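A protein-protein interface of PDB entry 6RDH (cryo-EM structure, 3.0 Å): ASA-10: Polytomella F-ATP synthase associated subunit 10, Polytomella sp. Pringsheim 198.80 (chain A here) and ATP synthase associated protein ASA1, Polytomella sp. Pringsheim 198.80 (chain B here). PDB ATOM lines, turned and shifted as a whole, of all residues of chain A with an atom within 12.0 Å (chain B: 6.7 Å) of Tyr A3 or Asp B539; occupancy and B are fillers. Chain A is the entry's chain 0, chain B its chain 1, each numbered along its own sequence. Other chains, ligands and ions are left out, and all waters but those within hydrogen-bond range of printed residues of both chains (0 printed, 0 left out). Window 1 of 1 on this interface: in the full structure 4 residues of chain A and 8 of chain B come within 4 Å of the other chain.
The backbone carbonyl oxygen (O) of Ser A2 sits close to the side-chain carboxylate (OD2) of Asp B539.
OG of Ser A4 sits close to O of Ser B317 (3.4 Å).
ND1 of His B535 lies within hydrogen-bond range of OD1 of Asp B539.
The backbone carbonyl oxygen (O) of His B535 is in hydrogen-bond range of the backbone NH (N) of Leu B540 (3.0 Å).
Ser A2 touches His B535 (CB to CE1, 3.99 Å).
Tyr A3 touches His B531 (OH to CE1, 3.2 Å).
O of Asp B539 touches CB of Tyr A3 (3.3 Å).
Tyr A3 touches Leu B540.
Tyr A3 touches Pro B541 (CD2 to CD, 3.8 Å).
Tyr A3 touches Val B544.
Pro B319 touches Ser A4 (CG to CA, 3.9 Å).
CD2 of Phe A7 touches CG of Pro B319 (3.7 Å).
Asp B539 touches Phe A7 (O to CE2, 3.2 Å).
Pro B541 touches Phe A7 (CB to CZ, 3.6 Å).
Asp B539 touches just these residues of chain A: Ser A2, Tyr A3 and Phe A7.
Ser B318 touches none of the printed residues of chain A.
No residue of chain A comes within 4 Å of Ile B538.
Leu B540 touches just one residue of chain A: Tyr A3.
Of chain A, only Tyr A3 (3.8 Å) and Phe A7 (3.6 Å) come within 4 Å of Pro B541.
Of the printed residues of chain A, Val B544 touches Tyr A3 (3.5 Å).
Printed residues of chain B within 4 Å of Ser A4: Ser B317 (3.3 Å) and Pro B319 (3.9 Å).
Of the printed residues of chain A, Pro B319 touches Ser A4 (3.9 Å) and Phe A7 (3.7 Å).
Printed residues of chain B within 4 Å of Phe A7: Pro B319 (3.7 Å), Asp B539 (3.2 Å) and Pro B541 (3.6 Å).
The nearest residue of chain B that does not touch Tyr A3 is Pro B319 (4.7 Å).
The nearest residue of chain A that does not touch Asp B539 is Ser A4 (4.8 Å).
Of the 10 printed residues of chain A, 4 touch a printed residue of chain B.
Hydrophobic or aromatic side chains of chain A that line the printed part of chain B: Tyr A3 and Phe A7.
Hydrophobic or aromatic side chains of chain B within 4 Å of the printed part of chain A: Pro B319, His B531, His B535, Leu B540, Pro B541 and Val B544.
Among the printed residues, 13 pairs touch across the chains.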
ATOM      1  N   SER A   2     -28.127 -13.695 -18.069  1.00  0.00           N
ATOM      2  CA  SER A   2     -28.254 -13.488 -16.640  1.00  0.00           C
ATOM      3  C   SER A   2     -27.078 -12.689 -16.131  1.00  0.00           C
ATOM      4  O   SER A   2     -26.268 -13.199 -15.371  1.00  0.00           O
ATOM      5  CB  SER A   2     -28.354 -14.822 -15.915  1.00  0.00           C
ATOM      6  OG  SER A   2     -29.669 -15.336 -16.007  1.00  0.00           O
ATOM      7  N   TYR A   3     -26.963 -11.459 -16.639  1.00  0.00           N
ATOM      8  CA  TYR A   3     -26.050 -10.393 -16.216  1.00  0.00           C
ATOM      9  C   TYR A   3     -24.582 -10.663 -16.492  1.00  0.00           C
ATOM     10  O   TYR A   3     -23.758  -9.777 -16.283  1.00  0.00           O
ATOM     11  CB  TYR A   3     -26.190 -10.082 -14.729  1.00  0.00           C
ATOM     12  CG  TYR A   3     -27.422  -9.324 -14.372  1.00  0.00           C
ATOM     13  CD1 TYR A   3     -27.882  -8.312 -15.172  1.00  0.00           C
ATOM     14  CD2 TYR A   3     -28.128  -9.632 -13.231  1.00  0.00           C
ATOM     15  CE1 TYR A   3     -29.014  -7.640 -14.857  1.00  0.00           C
ATOM     16  CE2 TYR A   3     -29.254  -8.957 -12.903  1.00  0.00           C
ATOM     17  CZ  TYR A   3     -29.696  -7.962 -13.721  1.00  0.00           C
ATOM     18  OH  TYR A   3     -30.834  -7.272 -13.407  1.00  0.00           O
ATOM     19  N   SER A   4     -24.232 -11.849 -16.971  1.00  0.00           N
ATOM     20  CA  SER A   4     -22.836 -12.137 -17.255  1.00  0.00           C
ATOM     21  C   SER A   4     -22.362 -11.429 -18.506  1.00  0.00           C
ATOM     22  O   SER A   4     -21.176 -11.120 -18.628  1.00  0.00           O
ATOM     23  CB  SER A   4     -22.628 -13.632 -17.410  1.00  0.00           C
ATOM     24  OG  SER A   4     -21.310 -13.898 -17.835  1.00  0.00           O
ATOM     25  N   ALA A   5     -23.264 -11.172 -19.434  1.00  0.00           N
ATOM     26  CA  ALA A   5     -22.948 -10.492 -20.673  1.00  0.00           C
ATOM     27  C   ALA A   5     -23.109  -8.992 -20.570  1.00  0.00           C
ATOM     28  O   ALA A   5     -22.870  -8.289 -21.552  1.00  0.00           O
ATOM     29  CB  ALA A   5     -23.832 -11.028 -21.790  1.00  0.00           C
ATOM     30  N   TYR A   6     -23.526  -8.489 -19.418  1.00  0.00           N
ATOM     31  CA  TYR A   6     -23.546  -7.052 -19.212  1.00  0.00           C
ATOM     32  C   TYR A   6     -22.200  -6.550 -18.732  1.00  0.00           C
ATOM     33  O   TYR A   6     -21.809  -5.428 -19.059  1.00  0.00           O
ATOM     34  CB  TYR A   6     -24.639  -6.690 -18.216  1.00  0.00           C
ATOM     35  CG  TYR A   6     -24.568  -5.289 -17.692  1.00  0.00           C
ATOM     36  CD1 TYR A   6     -24.752  -4.211 -18.527  1.00  0.00           C
ATOM     37  CD2 TYR A   6     -24.328  -5.049 -16.359  1.00  0.00           C
ATOM     38  CE1 TYR A   6     -24.687  -2.934 -18.045  1.00  0.00           C
ATOM     39  CE2 TYR A   6     -24.266  -3.785 -15.872  1.00  0.00           C
ATOM     40  CZ  TYR A   6     -24.446  -2.729 -16.714  1.00  0.00           C
ATOM     41  OH  TYR A   6     -24.382  -1.451 -16.224  1.00  0.00           O
ATOM     42  N   PHE A   7     -21.472  -7.367 -17.977  1.00  0.00           N
ATOM     43  CA  PHE A   7     -20.162  -6.959 -17.501  1.00  0.00           C
ATOM     44  C   PHE A   7     -19.079  -7.175 -18.533  1.00  0.00           C
ATOM     45  O   PHE A   7     -18.045  -6.507 -18.471  1.00  0.00           O
ATOM     46  CB  PHE A   7     -19.815  -7.705 -16.224  1.00  0.00           C
ATOM     47  CG  PHE A   7     -20.758  -7.435 -15.121  1.00  0.00           C
ATOM     48  CD1 PHE A   7     -20.949  -6.149 -14.662  1.00  0.00           C
ATOM     49  CD2 PHE A   7     -21.465  -8.455 -14.549  1.00  0.00           C
ATOM     50  CE1 PHE A   7     -21.827  -5.903 -13.660  1.00  0.00           C
ATOM     51  CE2 PHE A   7     -22.341  -8.209 -13.552  1.00  0.00           C
ATOM     52  CZ  PHE A   7     -22.521  -6.938 -13.103  1.00  0.00           C
ATOM     53  N   ALA A   8     -19.297  -8.073 -19.488  1.00  0.00           N
ATOM     54  CA  ALA A   8     -18.347  -8.234 -20.573  1.00  0.00           C
ATOM     55  C   ALA A   8     -18.396  -7.073 -21.553  1.00  0.00           C
ATOM     56  O   ALA A   8     -17.468  -6.917 -22.350  1.00  0.00           O
ATOM     57  CB  ALA A   8     -18.607  -9.548 -21.297  1.00  0.00           C
ATOM     58  N   LYS A   9     -19.453  -6.264 -21.515  1.00  0.00           N
ATOM     59  CA  LYS A   9     -19.547  -5.114 -22.404  1.00  0.00           C
ATOM     60  C   LYS A   9     -18.546  -4.039 -22.016  1.00  0.00           C
ATOM     61  O   LYS A   9     -17.848  -3.490 -22.873  1.00  0.00           O
ATOM     62  CB  LYS A   9     -20.964  -4.549 -22.387  1.00  0.00           C
ATOM     63  CG  LYS A   9     -21.985  -5.439 -23.052  1.00  0.00           C
ATOM     64  CD  LYS A   9     -23.336  -4.758 -23.102  1.00  0.00           C
ATOM     65  CE  LYS A   9     -24.392  -5.671 -23.676  1.00  0.00           C
ATOM     66  NZ  LYS A   9     -25.682  -4.967 -23.801  1.00  0.00           N
ATOM     67  N   ALA A  10     -18.473  -3.712 -20.736  1.00  0.00           N
ATOM     68  CA  ALA A  10     -17.475  -2.767 -20.260  1.00  0.00           C
ATOM     69  C   ALA A  10     -16.133  -3.475 -20.201  1.00  0.00           C
ATOM     70  O   ALA A  10     -15.993  -4.492 -19.517  1.00  0.00           O
ATOM     71  CB  ALA A  10     -17.862  -2.215 -18.893  1.00  0.00           C
ATOM     72  N   GLY A  11     -15.153  -2.953 -20.923  1.00  0.00           N
ATOM     73  CA  GLY A  11     -13.879  -3.630 -20.998  1.00  0.00           C
ATOM     74  C   GLY A  11     -12.978  -3.321 -19.827  1.00  0.00           C
ATOM     75  O   GLY A  11     -13.440  -3.193 -18.692  1.00  0.00           O
ATOM     76  N   ARG B 314     -25.377 -21.480 -10.907  1.00  0.00           N
ATOM     77  CA  ARG B 314     -25.433 -20.058 -11.204  1.00  0.00           C
ATOM     78  C   ARG B 314     -24.078 -19.398 -11.074  1.00  0.00           C
ATOM     79  O   ARG B 314     -23.819 -18.402 -11.751  1.00  0.00           O
ATOM     80  CB  ARG B 314     -26.422 -19.354 -10.279  1.00  0.00           C
ATOM     81  CG  ARG B 314     -27.864 -19.654 -10.564  1.00  0.00           C
ATOM     82  CD  ARG B 314     -28.764 -18.693  -9.851  1.00  0.00           C
ATOM     83  NE  ARG B 314     -28.439 -18.600  -8.438  1.00  0.00           N
ATOM     84  CZ  ARG B 314     -29.053 -19.287  -7.488  1.00  0.00           C
ATOM     85  NH1 ARG B 314     -30.023 -20.121  -7.800  1.00  0.00           N
ATOM     86  NH2 ARG B 314     -28.696 -19.137  -6.228  1.00  0.00           N
ATOM     87  N   LEU B 315     -23.217 -19.923 -10.202  1.00  0.00           N
ATOM     88  CA  LEU B 315     -21.847 -19.440 -10.114  1.00  0.00           C
ATOM     89  C   LEU B 315     -21.036 -19.814 -11.341  1.00  0.00           C
ATOM     90  O   LEU B 315     -20.100 -19.097 -11.697  1.00  0.00           O
ATOM     91  CB  LEU B 315     -21.164 -20.005  -8.876  1.00  0.00           C
ATOM     92  CG  LEU B 315     -21.054 -19.132  -7.642  1.00  0.00           C
ATOM     93  CD1 LEU B 315     -20.204 -19.829  -6.634  1.00  0.00           C
ATOM     94  CD2 LEU B 315     -20.454 -17.810  -7.997  1.00  0.00           C
ATOM     95  N   SER B 317     -22.041 -19.781 -14.394  1.00  0.00           N
ATOM     96  CA  SER B 317     -22.366 -18.833 -15.442  1.00  0.00           C
ATOM     97  C   SER B 317     -21.991 -17.405 -15.088  1.00  0.00           C
ATOM     98  O   SER B 317     -22.250 -16.501 -15.883  1.00  0.00           O
ATOM     99  CB  SER B 317     -23.854 -18.900 -15.752  1.00  0.00           C
ATOM    100  OG  SER B 317     -24.240 -20.236 -15.996  1.00  0.00           O
ATOM    101  N   SER B 318     -21.401 -17.183 -13.918  1.00  0.00           N
ATOM    102  CA  SER B 318     -21.018 -15.857 -13.482  1.00  0.00           C
ATOM    103  C   SER B 318     -19.816 -15.376 -14.287  1.00  0.00           C
ATOM    104  O   SER B 318     -19.144 -16.177 -14.936  1.00  0.00           O
ATOM    105  CB  SER B 318     -20.696 -15.892 -11.993  1.00  0.00           C
ATOM    106  OG  SER B 318     -19.692 -16.843 -11.731  1.00  0.00           O
ATOM    107  N   PRO B 319     -19.527 -14.069 -14.283  1.00  0.00           N
ATOM    108  CA  PRO B 319     -18.316 -13.593 -14.963  1.00  0.00           C
ATOM    109  C   PRO B 319     -17.023 -14.060 -14.330  1.00  0.00           C
ATOM    110  O   PRO B 319     -15.973 -13.952 -14.968  1.00  0.00           O
ATOM    111  CB  PRO B 319     -18.440 -12.072 -14.868  1.00  0.00           C
ATOM    112  CG  PRO B 319     -19.859 -11.824 -14.744  1.00  0.00           C
ATOM    113  CD  PRO B 319     -20.417 -12.942 -13.951  1.00  0.00           C
ATOM    114  N   HIS B 531     -35.411 -11.471  -6.842  1.00  0.00           N
ATOM    115  CA  HIS B 531     -34.377 -11.175  -7.824  1.00  0.00           C
ATOM    116  C   HIS B 531     -33.042 -10.871  -7.165  1.00  0.00           C
ATOM    117  O   HIS B 531     -31.996 -11.331  -7.648  1.00  0.00           O
ATOM    118  CB  HIS B 531     -34.801 -10.008  -8.692  1.00  0.00           C
ATOM    119  CG  HIS B 531     -33.896  -9.772  -9.852  1.00  0.00           C
ATOM    120  ND1 HIS B 531     -33.081  -8.672  -9.944  1.00  0.00           N
ATOM    121  CD2 HIS B 531     -33.673 -10.500 -10.966  1.00  0.00           C
ATOM    122  CE1 HIS B 531     -32.401  -8.725 -11.069  1.00  0.00           C
ATOM    123  NE2 HIS B 531     -32.741  -9.825 -11.709  1.00  0.00           N
ATOM    124  N   LYS B 534     -31.636 -14.140  -5.831  1.00  0.00           N
ATOM    125  CA  LYS B 534     -31.180 -15.016  -6.896  1.00  0.00           C
ATOM    126  C   LYS B 534     -29.857 -14.550  -7.473  1.00  0.00           C
ATOM    127  O   LYS B 534     -29.040 -15.380  -7.876  1.00  0.00           O
ATOM    128  CB  LYS B 534     -32.249 -15.089  -7.981  1.00  0.00           C
ATOM    129  CG  LYS B 534     -31.986 -16.046  -9.107  1.00  0.00           C
ATOM    130  CD  LYS B 534     -32.943 -15.769 -10.234  1.00  0.00           C
ATOM    131  CE  LYS B 534     -32.578 -16.541 -11.478  1.00  0.00           C
ATOM    132  NZ  LYS B 534     -33.431 -16.133 -12.624  1.00  0.00           N
ATOM    133  N   HIS B 535     -29.605 -13.240  -7.492  1.00  0.00           N
ATOM    134  CA  HIS B 535     -28.430 -12.731  -8.179  1.00  0.00           C
ATOM    135  C   HIS B 535     -27.361 -12.112  -7.289  1.00  0.00           C
ATOM    136  O   HIS B 535     -26.282 -11.818  -7.797  1.00  0.00           O
ATOM    137  CB  HIS B 535     -28.855 -11.702  -9.224  1.00  0.00           C
ATOM    138  CG  HIS B 535     -29.454 -12.305 -10.449  1.00  0.00           C
ATOM    139  ND1 HIS B 535     -28.703 -12.669 -11.540  1.00  0.00           N
ATOM    140  CD2 HIS B 535     -30.732 -12.617 -10.752  1.00  0.00           C
ATOM    141  CE1 HIS B 535     -29.494 -13.174 -12.466  1.00  0.00           C
ATOM    142  NE2 HIS B 535     -30.731 -13.156 -12.012  1.00  0.00           N
ATOM    143  N   PHE B 536     -27.612 -11.905  -5.999  1.00  0.00           N
ATOM    144  CA  PHE B 536     -26.649 -11.225  -5.137  1.00  0.00           C
ATOM    145  C   PHE B 536     -25.442 -12.101  -4.876  1.00  0.00           C
ATOM    146  O   PHE B 536     -25.568 -13.296  -4.607  1.00  0.00           O
ATOM    147  CB  PHE B 536     -27.279 -10.859  -3.799  1.00  0.00           C
ATOM    148  CG  PHE B 536     -26.467  -9.929  -2.972  1.00  0.00           C
ATOM    149  CD1 PHE B 536     -26.456  -8.583  -3.240  1.00  0.00           C
ATOM    150  CD2 PHE B 536     -25.746 -10.397  -1.899  1.00  0.00           C
ATOM    151  CE1 PHE B 536     -25.723  -7.734  -2.476  1.00  0.00           C
ATOM    152  CE2 PHE B 536     -25.016  -9.546  -1.139  1.00  0.00           C
ATOM    153  CZ  PHE B 536     -25.005  -8.217  -1.428  1.00  0.00           C
ATOM    154  N   GLY B 537     -24.264 -11.495  -4.946  1.00  0.00           N
ATOM    155  CA  GLY B 537     -23.040 -12.215  -4.710  1.00  0.00           C
ATOM    156  C   GLY B 537     -22.631 -13.129  -5.829  1.00  0.00           C
ATOM    157  O   GLY B 537     -21.698 -13.912  -5.655  1.00  0.00           O
ATOM    158  N   ILE B 538     -23.324 -13.086  -6.960  1.00  0.00           N
ATOM    159  CA  ILE B 538     -22.955 -13.876  -8.120  1.00  0.00           C
ATOM    160  C   ILE B 538     -22.748 -12.937  -9.290  1.00  0.00           C
ATOM    161  O   ILE B 538     -21.623 -12.765  -9.764  1.00  0.00           O
ATOM    162  CB  ILE B 538     -24.032 -14.921  -8.443  1.00  0.00           C
ATOM    163  CG1 ILE B 538     -24.204 -15.895  -7.292  1.00  0.00           C
ATOM    164  CG2 ILE B 538     -23.666 -15.672  -9.671  1.00  0.00           C
ATOM    165  CD1 ILE B 538     -25.345 -16.808  -7.477  1.00  0.00           C
ATOM    166  N   ASP B 539     -23.812 -12.282  -9.739  1.00  0.00           N
ATOM    167  CA  ASP B 539     -23.668 -11.396 -10.883  1.00  0.00           C
ATOM    168  C   ASP B 539     -24.543 -10.158 -10.835  1.00  0.00           C
ATOM    169  O   ASP B 539     -24.691  -9.511 -11.866  1.00  0.00           O
ATOM    170  CB  ASP B 539     -23.928 -12.142 -12.203  1.00  0.00           C
ATOM    171  CG  ASP B 539     -25.196 -12.995 -12.189  1.00  0.00           C
ATOM    172  OD1 ASP B 539     -26.226 -12.580 -11.634  1.00  0.00           O
ATOM    173  OD2 ASP B 539     -25.169 -14.099 -12.766  1.00  0.00           O
ATOM    174  N   LEU B 540     -25.133  -9.815  -9.715  1.00  0.00           N
ATOM    175  CA  LEU B 540     -26.024  -8.665  -9.689  1.00  0.00           C
ATOM    176  C   LEU B 540     -25.205  -7.390  -9.716  1.00  0.00           C
ATOM    177  O   LEU B 540     -24.299  -7.240  -8.905  1.00  0.00           O
ATOM    178  CB  LEU B 540     -26.880  -8.688  -8.439  1.00  0.00           C
ATOM    179  CG  LEU B 540     -28.052  -7.744  -8.209  1.00  0.00           C
ATOM    180  CD1 LEU B 540     -29.012  -7.791  -9.336  1.00  0.00           C
ATOM    181  CD2 LEU B 540     -28.740  -8.171  -6.970  1.00  0.00           C
ATOM    182  N   PRO B 541     -25.457  -6.475 -10.638  1.00  0.00           N
ATOM    183  CA  PRO B 541     -24.739  -5.211 -10.605  1.00  0.00           C
ATOM    184  C   PRO B 541     -25.250  -4.310  -9.502  1.00  0.00           C
ATOM    185  O   PRO B 541     -26.334  -4.492  -8.958  1.00  0.00           O
ATOM    186  CB  PRO B 541     -24.998  -4.610 -11.983  1.00  0.00           C
ATOM    187  CG  PRO B 541     -26.069  -5.314 -12.516  1.00  0.00           C
ATOM    188  CD  PRO B 541     -26.170  -6.636 -11.903  1.00  0.00           C
ATOM    189  N   VAL B 544     -28.488  -2.194 -10.499  1.00  0.00           N
ATOM    190  CA  VAL B 544     -29.781  -2.839 -10.346  1.00  0.00           C
ATOM    191  C   VAL B 544     -30.190  -2.873  -8.885  1.00  0.00           C
ATOM    192  O   VAL B 544     -31.372  -2.743  -8.565  1.00  0.00           O
ATOM    193  CB  VAL B 544     -29.714  -4.229 -10.991  1.00  0.00           C
ATOM    194  CG1 VAL B 544     -30.984  -4.945 -10.860  1.00  0.00           C
ATOM    195  CG2 VAL B 544     -29.458  -4.055 -12.439  1.00  0.00           C
ATOM    196  N   MET B 548     -33.578  -1.077  -7.724  1.00  0.00           N
ATOM    197  CA  MET B 548     -34.605  -1.815  -7.006  1.00  0.00           C
ATOM    198  C   MET B 548     -34.820  -1.262  -5.608  1.00  0.00           C
ATOM    199  O   MET B 548     -35.956  -1.171  -5.140  1.00  0.00           O
ATOM    200  CB  MET B 548     -34.210  -3.278  -6.917  1.00  0.00           C
ATOM    201  CG  MET B 548     -34.886  -4.160  -7.896  1.00  0.00           C
ATOM    202  SD  MET B 548     -34.541  -5.858  -7.498  1.00  0.00           S
ATOM    203  CE  MET B 548     -32.820  -5.854  -7.866  1.00  0.00           C
